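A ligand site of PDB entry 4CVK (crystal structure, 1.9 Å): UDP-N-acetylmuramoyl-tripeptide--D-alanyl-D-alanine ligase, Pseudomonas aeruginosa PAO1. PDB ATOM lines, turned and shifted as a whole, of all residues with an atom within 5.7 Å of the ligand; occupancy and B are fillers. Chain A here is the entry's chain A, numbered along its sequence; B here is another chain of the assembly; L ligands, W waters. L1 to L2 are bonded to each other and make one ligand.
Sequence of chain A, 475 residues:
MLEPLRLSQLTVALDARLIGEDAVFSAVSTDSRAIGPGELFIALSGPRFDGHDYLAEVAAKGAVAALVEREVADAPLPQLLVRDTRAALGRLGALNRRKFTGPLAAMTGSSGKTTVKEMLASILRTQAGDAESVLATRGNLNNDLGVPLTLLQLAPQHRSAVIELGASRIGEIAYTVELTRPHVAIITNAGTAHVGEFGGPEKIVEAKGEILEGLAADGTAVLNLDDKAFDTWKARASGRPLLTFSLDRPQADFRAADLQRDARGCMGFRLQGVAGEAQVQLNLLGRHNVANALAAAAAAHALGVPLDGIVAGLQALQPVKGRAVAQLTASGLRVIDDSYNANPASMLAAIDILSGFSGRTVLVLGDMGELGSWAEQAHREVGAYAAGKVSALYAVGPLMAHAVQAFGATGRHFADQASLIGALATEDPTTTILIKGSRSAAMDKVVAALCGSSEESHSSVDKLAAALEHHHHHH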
ATOM      1  N   THR A  30     -22.427  24.471  13.827  1.00  0.00           N
ATOM      2  CA  THR A  30     -21.659  24.752  12.608  1.00  0.00           C
ATOM      3  C   THR A  30     -22.549  25.177  11.434  1.00  0.00           C
ATOM      4  O   THR A  30     -22.140  25.081  10.279  1.00  0.00           O
ATOM      5  CB  THR A  30     -20.861  23.488  12.162  1.00  0.00           C
ATOM      6  OG1 THR A  30     -21.783  22.413  11.988  1.00  0.00           O
ATOM      7  CG2 THR A  30     -19.865  23.081  13.187  1.00  0.00           C
ATOM      8  N   ASP A  31     -23.771  25.645  11.703  1.00  0.00           N
ATOM      9  CA  ASP A  31     -24.733  25.848  10.619  1.00  0.00           C
ATOM     10  C   ASP A  31     -25.716  26.926  11.009  1.00  0.00           C
ATOM     11  O   ASP A  31     -26.466  26.796  11.988  1.00  0.00           O
ATOM     12  CB  ASP A  31     -25.444  24.535  10.308  1.00  0.00           C
ATOM     13  CG  ASP A  31     -26.217  24.570   9.027  1.00  0.00           C
ATOM     14  OD1 ASP A  31     -26.613  25.682   8.593  1.00  0.00           O
ATOM     15  OD2 ASP A  31     -26.388  23.480   8.415  1.00  0.00           O
ATOM     16  N   SER A  32     -25.703  28.018  10.239  1.00  0.00           N
ATOM     17  CA  SER A  32     -26.561  29.169  10.520  1.00  0.00           C
ATOM     18  C   SER A  32     -28.029  28.846  10.331  1.00  0.00           C
ATOM     19  O   SER A  32     -28.879  29.582  10.810  1.00  0.00           O
ATOM     20  CB  SER A  32     -26.163  30.373   9.643  1.00  0.00           C
ATOM     21  OG  SER A  32     -26.463  30.127   8.272  1.00  0.00           O
ATOM     22  N   ARG A  33     -28.340  27.731   9.657  1.00  0.00           N
ATOM     23  CA  ARG A  33     -29.709  27.258   9.478  1.00  0.00           C
ATOM     24  C   ARG A  33     -30.261  26.465  10.697  1.00  0.00           C
ATOM     25  O   ARG A  33     -31.430  26.112  10.732  1.00  0.00           O
ATOM     26  CB  ARG A  33     -29.785  26.416   8.196  1.00  0.00           C
ATOM     27  CG  ARG A  33     -29.316  27.176   6.944  1.00  0.00           C
ATOM     28  CD  ARG A  33     -29.009  26.253   5.790  1.00  0.00           C
ATOM     29  NE  ARG A  33     -27.814  25.449   6.016  1.00  0.00           N
ATOM     30  CZ  ARG A  33     -27.217  24.686   5.093  1.00  0.00           C
ATOM     31  NH1 ARG A  33     -27.651  24.674   3.831  1.00  0.00           N
ATOM     32  NH2 ARG A  33     -26.140  23.985   5.395  1.00  0.00           N
ATOM     33  N   PHE A  41     -21.289  29.941  17.186  1.00  0.00           N
ATOM     34  CA  PHE A  41     -21.269  29.510  15.774  1.00  0.00           C
ATOM     35  C   PHE A  41     -19.829  29.217  15.377  1.00  0.00           C
ATOM     36  O   PHE A  41     -18.956  29.986  15.697  1.00  0.00           O
ATOM     37  CB  PHE A  41     -21.797  30.629  14.859  1.00  0.00           C
ATOM     38  CG  PHE A  41     -21.696  30.333  13.382  1.00  0.00           C
ATOM     39  CD1 PHE A  41     -22.268  29.175  12.828  1.00  0.00           C
ATOM     40  CD2 PHE A  41     -21.047  31.218  12.529  1.00  0.00           C
ATOM     41  CE1 PHE A  41     -22.187  28.917  11.457  1.00  0.00           C
ATOM     42  CE2 PHE A  41     -21.001  30.987  11.161  1.00  0.00           C
ATOM     43  CZ  PHE A  41     -21.572  29.846  10.622  1.00  0.00           C
ATOM     44  N   ILE A  42     -19.603  28.116  14.677  1.00  0.00           N
ATOM     45  CA  ILE A  42     -18.277  27.792  14.185  1.00  0.00           C
ATOM     46  C   ILE A  42     -18.338  27.883  12.668  1.00  0.00           C
ATOM     47  O   ILE A  42     -19.095  27.158  12.035  1.00  0.00           O
ATOM     48  CB  ILE A  42     -17.824  26.376  14.600  1.00  0.00           C
ATOM     49  CG1 ILE A  42     -17.787  26.265  16.138  1.00  0.00           C
ATOM     50  CG2 ILE A  42     -16.445  26.089  14.032  1.00  0.00           C
ATOM     51  CD1 ILE A  42     -17.390  24.907  16.644  1.00  0.00           C
ATOM     52  N   LEU A  44     -17.111  27.139   9.189  1.00  0.00           N
ATOM     53  CA  LEU A  44     -16.344  26.209   8.386  1.00  0.00           C
ATOM     54  C   LEU A  44     -16.441  26.564   6.914  1.00  0.00           C
ATOM     55  O   LEU A  44     -17.519  26.857   6.393  1.00  0.00           O
ATOM     56  CB  LEU A  44     -16.873  24.785   8.573  1.00  0.00           C
ATOM     57  CG  LEU A  44     -16.848  24.268  10.012  1.00  0.00           C
ATOM     58  CD1 LEU A  44     -17.482  22.879  10.151  1.00  0.00           C
ATOM     59  CD2 LEU A  44     -15.412  24.246  10.537  1.00  0.00           C
ATOM     60  N   SER A  45     -15.312  26.456   6.250  1.00  0.00           N
ATOM     61  CA  SER A  45     -15.245  26.664   4.814  1.00  0.00           C
ATOM     62  C   SER A  45     -15.514  25.348   4.133  1.00  0.00           C
ATOM     63  O   SER A  45     -14.916  24.359   4.485  1.00  0.00           O
ATOM     64  CB  SER A  45     -13.826  27.147   4.493  1.00  0.00           C
ATOM     65  OG  SER A  45     -13.726  27.485   3.140  1.00  0.00           O
ATOM     66  N   GLY A  46     -16.423  25.281   3.170  1.00  0.00           N
ATOM     67  CA  GLY A  46     -16.718  24.006   2.497  1.00  0.00           C
ATOM     68  C   GLY A  46     -16.630  24.049   0.965  1.00  0.00           C
ATOM     69  O   GLY A  46     -16.253  25.078   0.404  1.00  0.00           O
ATOM     70  N   PRO A  47     -17.025  22.949   0.292  1.00  0.00           N
ATOM     71  CA  PRO A  47     -16.956  22.912  -1.182  1.00  0.00           C
ATOM     72  C   PRO A  47     -18.049  23.714  -1.853  1.00  0.00           C
ATOM     73  O   PRO A  47     -17.924  24.022  -3.021  1.00  0.00           O
ATOM     74  CB  PRO A  47     -17.133  21.431  -1.529  1.00  0.00           C
ATOM     75  CG  PRO A  47     -17.281  20.696  -0.231  1.00  0.00           C
ATOM     76  CD  PRO A  47     -17.561  21.694   0.845  1.00  0.00           C
ATOM     77  N   ARG A  48     -19.129  24.023  -1.127  1.00  0.00           N
ATOM     78  CA  ARG A  48     -20.242  24.779  -1.656  1.00  0.00           C
ATOM     79  C   ARG A  48     -20.425  26.125  -0.945  1.00  0.00           C
ATOM     80  O   ARG A  48     -20.698  27.130  -1.607  1.00  0.00           O
ATOM     81  CB  ARG A  48     -21.523  23.952  -1.584  1.00  0.00           C
ATOM     82  N   PHE A  49     -20.295  26.169   0.377  1.00  0.00           N
ATOM     83  CA  PHE A  49     -20.513  27.389   1.123  1.00  0.00           C
ATOM     84  C   PHE A  49     -19.343  27.660   2.062  1.00  0.00           C
ATOM     85  O   PHE A  49     -18.471  26.817   2.291  1.00  0.00           O
ATOM     86  CB  PHE A  49     -21.815  27.301   1.974  1.00  0.00           C
ATOM     87  CG  PHE A  49     -23.036  26.937   1.189  1.00  0.00           C
ATOM     88  CD1 PHE A  49     -23.562  27.828   0.251  1.00  0.00           C
ATOM     89  CD2 PHE A  49     -23.669  25.724   1.384  1.00  0.00           C
ATOM     90  CE1 PHE A  49     -24.689  27.505  -0.484  1.00  0.00           C
ATOM     91  CE2 PHE A  49     -24.791  25.388   0.665  1.00  0.00           C
ATOM     92  CZ  PHE A  49     -25.308  26.276  -0.284  1.00  0.00           C
ATOM     93  N   ASP A  50     -19.321  28.876   2.579  1.00  0.00           N
ATOM     94  CA  ASP A  50     -18.345  29.293   3.551  1.00  0.00           C
ATOM     95  C   ASP A  50     -19.113  29.838   4.714  1.00  0.00           C
ATOM     96  O   ASP A  50     -19.757  30.897   4.589  1.00  0.00           O
ATOM     97  CB  ASP A  50     -17.432  30.382   3.000  1.00  0.00           C
ATOM     98  CG  ASP A  50     -16.378  30.777   3.984  1.00  0.00           C
ATOM     99  OD1 ASP A  50     -16.394  30.295   5.150  1.00  0.00           O
ATOM    100  OD2 ASP A  50     -15.506  31.596   3.606  1.00  0.00           O
ATOM    101  N   GLY A  51     -19.041  29.147   5.830  1.00  0.00           N
ATOM    102  CA  GLY A  51     -19.691  29.604   7.062  1.00  0.00           C
ATOM    103  C   GLY A  51     -19.428  31.047   7.459  1.00  0.00           C
ATOM    104  O   GLY A  51     -20.253  31.669   8.105  1.00  0.00           O
ATOM    105  N   TYR A  54     -22.088  34.037   7.037  1.00  0.00           N
ATOM    106  CA  TYR A  54     -23.413  34.034   7.647  1.00  0.00           C
ATOM    107  C   TYR A  54     -23.415  34.651   9.043  1.00  0.00           C
ATOM    108  O   TYR A  54     -24.233  34.278   9.870  1.00  0.00           O
ATOM    109  CB  TYR A  54     -23.961  32.597   7.700  1.00  0.00           C
ATOM    110  CG  TYR A  54     -24.076  32.012   6.312  1.00  0.00           C
ATOM    111  CD1 TYR A  54     -25.193  32.246   5.503  1.00  0.00           C
ATOM    112  CD2 TYR A  54     -23.043  31.243   5.786  1.00  0.00           C
ATOM    113  CE1 TYR A  54     -25.271  31.718   4.208  1.00  0.00           C
ATOM    114  CE2 TYR A  54     -23.129  30.721   4.510  1.00  0.00           C
ATOM    115  CZ  TYR A  54     -24.231  30.959   3.731  1.00  0.00           C
ATOM    116  OH  TYR A  54     -24.231  30.431   2.472  1.00  0.00           O
ATOM    117  N   GLU A  57     -26.694  36.476   9.993  1.00  0.00           N
ATOM    118  CA  GLU A  57     -27.780  35.547  10.275  1.00  0.00           C
ATOM    119  C   GLU A  57     -27.652  34.930  11.681  1.00  0.00           C
ATOM    120  O   GLU A  57     -28.594  34.931  12.438  1.00  0.00           O
ATOM    121  CB  GLU A  57     -27.899  34.478   9.192  1.00  0.00           C
ATOM    122  CG  GLU A  57     -28.924  33.401   9.509  1.00  0.00           C
ATOM    123  CD  GLU A  57     -29.123  32.362   8.410  1.00  0.00           C
ATOM    124  OE1 GLU A  57     -28.183  32.079   7.610  1.00  0.00           O
ATOM    125  OE2 GLU A  57     -30.240  31.805   8.373  1.00  0.00           O
ATOM    126  N   ARG A  86     -11.609  23.890  11.704  1.00  0.00           N
ATOM    127  CA  ARG A  86     -11.749  22.424  11.838  1.00  0.00           C
ATOM    128  C   ARG A  86     -10.962  21.895  13.034  1.00  0.00           C
ATOM    129  O   ARG A  86     -11.502  21.116  13.842  1.00  0.00           O
ATOM    130  CB  ARG A  86     -11.290  21.676  10.595  1.00  0.00           C
ATOM    131  CG  ARG A  86     -12.057  22.039   9.359  1.00  0.00           C
ATOM    132  CD  ARG A  86     -11.777  21.021   8.259  1.00  0.00           C
ATOM    133  NE  ARG A  86     -12.807  21.217   7.251  1.00  0.00           N
ATOM    134  CZ  ARG A  86     -13.662  20.304   6.838  1.00  0.00           C
ATOM    135  NH1 ARG A  86     -13.602  19.051   7.277  1.00  0.00           N
ATOM    136  NH2 ARG A  86     -14.556  20.668   5.952  1.00  0.00           N
ATOM    137  N   ASN A 143     -17.026  11.619  11.486  1.00  0.00           N
ATOM    138  CA  ASN A 143     -15.755  11.976  10.829  1.00  0.00           C
ATOM    139  C   ASN A 143     -14.998  13.051  11.619  1.00  0.00           C
ATOM    140  O   ASN A 143     -15.337  13.301  12.789  1.00  0.00           O
ATOM    141  CB  ASN A 143     -15.961  12.353   9.337  1.00  0.00           C
ATOM    142  CG  ASN A 143     -16.709  13.656   9.139  1.00  0.00           C
ATOM    143  OD1 ASN A 143     -16.925  14.421  10.068  1.00  0.00           O
ATOM    144  ND2 ASN A 143     -17.098  13.907   7.903  1.00  0.00           N
ATOM    145  N   ASP A 144     -13.950  13.634  11.019  1.00  0.00           N
ATOM    146  CA  ASP A 144     -13.158  14.641  11.703  1.00  0.00           C
ATOM    147  C   ASP A 144     -13.968  15.866  12.221  1.00  0.00           C
ATOM    148  O   ASP A 144     -13.458  16.568  13.074  1.00  0.00           O
ATOM    149  CB  ASP A 144     -11.943  15.104  10.876  1.00  0.00           C
ATOM    150  CG  ASP A 144     -12.338  15.663   9.477  1.00  0.00           C
ATOM    151  OD1 ASP A 144     -13.513  15.650   9.127  1.00  0.00           O
ATOM    152  OD2 ASP A 144     -11.427  16.023   8.701  1.00  0.00           O
ATOM    153  N   LEU A 145     -15.173  16.104  11.692  1.00  0.00           N
ATOM    154  CA  LEU A 145     -16.106  17.103  12.241  1.00  0.00           C
ATOM    155  C   LEU A 145     -17.189  16.447  13.116  1.00  0.00           C
ATOM    156  O   LEU A 145     -17.536  16.980  14.145  1.00  0.00           O
ATOM    157  CB  LEU A 145     -16.803  17.916  11.124  1.00  0.00           C
ATOM    158  CG  LEU A 145     -15.901  18.522  10.037  1.00  0.00           C
ATOM    159  CD1 LEU A 145     -16.721  19.283   8.998  1.00  0.00           C
ATOM    160  CD2 LEU A 145     -14.826  19.427  10.661  1.00  0.00           C
ATOM    161  N   ALA B   1     -20.389  16.435   7.924  1.00  0.00           N
ATOM    162  CA  ALA B   1     -19.890  15.861   9.199  1.00  0.00           C
ATOM    163  C   ALA B   1     -20.382  14.436   9.416  1.00  0.00           C
ATOM    164  O   ALA B   1     -20.025  13.832  10.423  1.00  0.00           O
ATOM    165  CB  ALA B   1     -20.391  16.749  10.321  1.00  0.00           C
ATOM    166  N   FGA B   2     -21.204  13.909   8.465  1.00  0.00           N
ATOM    167  CA  FGA B   2     -21.790  12.582   8.649  1.00  0.00           C
ATOM    168  C   FGA B   2     -23.313  12.694   8.673  1.00  0.00           C
ATOM    169  O   FGA B   2     -23.772  13.830   8.442  1.00  0.00           O
ATOM    170  CB  FGA B   2     -21.389  11.649   7.555  1.00  0.00           C
ATOM    171  CG  FGA B   2     -19.971  11.203   7.804  1.00  0.00           C
ATOM    172  CD  FGA B   2     -19.603  10.032   6.902  1.00  0.00           C
ATOM    173  OE1 FGA B   2     -19.870  10.088   5.715  1.00  0.00           O
ATOM    174  OXT FGA B   2     -23.995  11.684   8.961  1.00  0.00           O
ATOM    175  C   API B   3     -18.671   6.481   7.131  1.00  0.00           C
ATOM    176  CA  API B   3     -18.372   7.903   6.607  1.00  0.00           C
ATOM    177  C3  API B   3     -16.857   8.148   6.574  1.00  0.00           C
ATOM    178  C4  API B   3     -16.597   9.667   6.285  1.00  0.00           C
ATOM    179  C5  API B   3     -15.094   9.988   6.254  1.00  0.00           C
ATOM    180  C6  API B   3     -14.791  11.495   5.966  1.00  0.00           C
ATOM    181  C7  API B   3     -15.648  12.094   4.846  1.00  0.00           C
ATOM    182  O   API B   3     -19.265   6.366   8.197  1.00  0.00           O
ATOM    183  OXT API B   3     -18.307   5.508   6.451  1.00  0.00           O
ATOM    184  O3  API B   3     -16.713  12.666   5.175  1.00  0.00           O
ATOM    185  O4  API B   3     -15.225  11.947   3.667  1.00  0.00           O
ATOM    186  N   API B   3     -18.924   8.994   7.440  1.00  0.00           N
ATOM    187  N6  API B   3     -13.384  11.609   5.584  1.00  0.00           N
HETATM  188  C1  LIG L   1     -23.365  20.742   5.150  1.00  0.00           C
HETATM  189  C2  LIG L   1     -22.336  19.830   5.885  1.00  0.00           C
HETATM  190  C3  LIG L   1     -22.265  18.484   5.185  1.00  0.00           C
HETATM  191  C4  LIG L   1     -23.667  17.909   5.019  1.00  0.00           C
HETATM  192  C5  LIG L   1     -24.550  18.896   4.250  1.00  0.00           C
HETATM  193  C6  LIG L   1     -25.847  18.201   3.918  1.00  0.00           C
HETATM  194  C7  LIG L   1     -20.166  20.554   6.861  1.00  0.00           C
HETATM  195  C8  LIG L   1     -18.853  21.298   6.593  1.00  0.00           C
HETATM  196  C9  LIG L   1     -20.193  17.297   5.684  1.00  0.00           C
HETATM  197  C10 LIG L   1     -19.557  16.674   6.923  1.00  0.00           C
HETATM  198  C11 LIG L   1     -20.104  16.269   4.530  1.00  0.00           C
HETATM  199  O1  LIG L   1     -22.827  20.955   3.841  1.00  0.00           O
HETATM  200  O2  LIG L   1     -21.552  17.590   6.008  1.00  0.00           O
HETATM  201  O3  LIG L   1     -23.565  16.704   4.267  1.00  0.00           O
HETATM  202  O4  LIG L   1     -24.667  20.131   5.057  1.00  0.00           O
HETATM  203  O5  LIG L   1     -26.452  17.981   5.194  1.00  0.00           O
HETATM  204  O6  LIG L   1     -20.373  20.028   7.945  1.00  0.00           O
HETATM  205  O7  LIG L   1     -18.356  16.425   6.989  1.00  0.00           O
HETATM  206  N1  LIG L   1     -21.027  20.488   5.817  1.00  0.00           N
HETATM  207  N1  LG2 L   2     -23.484  26.971   6.127  1.00  0.00           N
HETATM  208  C1  LG2 L   2     -24.150  27.831   6.917  1.00  0.00           C
HETATM  209  N2  LG2 L   2     -25.328  28.425   6.463  1.00  0.00           N
HETATM  210  C2  LG2 L   2     -25.804  28.154   5.184  1.00  0.00           C
HETATM  211  C3  LG2 L   2     -25.132  27.263   4.341  1.00  0.00           C
HETATM  212  C4  LG2 L   2     -23.979  26.663   4.822  1.00  0.00           C
HETATM  213  O1  LG2 L   2     -23.776  28.089   8.058  1.00  0.00           O
HETATM  214  O2  LG2 L   2     -26.838  28.720   4.826  1.00  0.00           O
HETATM  215  C5  LG2 L   2     -22.269  26.315   6.626  1.00  0.00           C
HETATM  216  C6  LG2 L   2     -22.506  24.829   6.712  1.00  0.00           C
HETATM  217  O3  LG2 L   2     -23.287  24.566   7.871  1.00  0.00           O
HETATM  218  C7  LG2 L   2     -21.106  24.289   6.763  1.00  0.00           C
HETATM  219  C8  LG2 L   2     -20.332  25.346   5.966  1.00  0.00           C
HETATM  220  O4  LG2 L   2     -21.185  26.442   5.670  1.00  0.00           O
HETATM  221  O5  LG2 L   2     -20.544  24.299   8.056  1.00  0.00           O
HETATM  222  C9  LG2 L   2     -19.803  24.766   4.688  1.00  0.00           C
HETATM  223  O6  LG2 L   2     -20.859  24.310   3.883  1.00  0.00           O
HETATM  224  P1  LG2 L   2     -20.575  23.121   2.822  1.00  0.00           P
HETATM  225  O7  LG2 L   2     -19.766  23.788   1.609  1.00  0.00           O
HETATM  226  O8  LG2 L   2     -19.801  21.976   3.397  1.00  0.00           O
HETATM  227  O9  LG2 L   2     -21.962  22.738   2.192  1.00  0.00           O
HETATM  228  P2  LG2 L   2     -23.284  22.237   2.959  1.00  0.00           P
HETATM  229  O10 LG2 L   2     -24.041  23.341   3.807  1.00  0.00           O
HETATM  230  O11 LG2 L   2     -24.189  21.708   1.995  1.00  0.00           O
HETATM  231  O   HOH W   1     -21.667  22.091   9.343  1.00  0.00           O
HETATM  232  O   HOH W   2     -23.400  16.441   8.530  1.00  0.00           O
HETATM  233  O   HOH W   3     -19.995  26.862   9.292  1.00  0.00           O
HETATM  234  O   HOH W   4     -24.189  21.575   8.236  1.00  0.00           O
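An oxygen (O10) of LG2 L2 is in salt-bridge range of the guanidinium group (NH2) of Arg 33 (2.7 Å). The backbone NH of Ala 1 of chain B is covalently linked to a carbon (C10) of LIG L1, at 1.3 Å. O of Thr 30 is in hydrogen-bond range of O3 of LG2 L2, 2.7 Å away. An oxygen (O1) of LG2 L2 lies within hydrogen-bond range of the backbone NH of Ser 32 (2.9 Å). The side-chain carboxylate of Asp 31 sits close to an oxygen (O3) of LG2 L2 (3.3 Å). N of Gly 51 is in hydrogen-bond range of O4 of LG2 L2 (3.5 Å). O7 of LG2 L2 lies within hydrogen-bond range of N of Arg 48 (2.8 Å). N of Phe 49 is in hydrogen-bond range of O7 of LG2 L2, at 2.7 Å. The side-chain hydroxyl of Ser 32 is in hydrogen-bond range of a nitrogen (N2) of LG2 L2 (2.7 Å). An oxygen (O7) of LIG L1 sits at hydrogen-bond distance from the side-chain amide nitrogen of Asn 143.
The backbone NH of Gly 51 is in hydrogen-bond range of the backbone carbonyl oxygen of Leu 44, 2.8 Å away. OG of Ser 32 sits at hydrogen-bond distance from OE1 of Glu 57, at 2.7 Å. The side-chain amide nitrogen (ND2) of Asn 143 lies within hydrogen-bond range of O3 of API 3 of chain B (3.0 Å). NE of Arg 33 lies within salt-bridge range of OD1 of Asp 31 (2.9 Å). The backbone NH of Leu 145 sits at hydrogen-bond distance from the side-chain amide oxygen of Asn 143, 2.9 Å away. The backbone carbonyl oxygen (O) of Ala 1 of chain B sits close to the side-chain amide oxygen (OD1) of Asn 143.
The backbone nitrogen (N) of Pro 47 sits close to an oxygen (O7) of LG2 L2 (3.2 Å). Merely in contact with the ligand: Gly 46, Leu 44, Tyr 54, FGA 2 of chain B, Leu 145 and Phe 41. 16 residues have an atom within 4 Å of the ligand: Thr 30, Asp 31, Ser 32, Arg 33, Phe 41, Leu 44, Gly 46, Pro 47, Arg 48, Phe 49, Gly 51, Tyr 54, Asn 143, Leu 145, Ala 1 of chain B and FGA 2 of chain B. The nearest printed residue that does not touch the ligand is Asp 50 (4.1 Å).
Water W1 lies within hydrogen-bond range of OG1 of Thr 30 and O5 of LG2 L2. Water W3 lies within hydrogen-bond range of an oxygen (O5) of LG2 L2 (2.9 Å), the backbone NH of Leu 44 (2.9 Å), the backbone carbonyl oxygen of Ile 42 (2.9 Å) and the backbone carbonyl oxygen of Thr 30 (3.0 Å). Water W4 bridges the side-chain carboxylate (OD2) of Asp 31 (2.9 Å) and an oxygen (O3) of LG2 L2 (3.1 Å). Water W2 lies within hydrogen-bond range of O of FGA 2 of chain B, N of Ala 1 of chain B and O2 of LIG L1.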
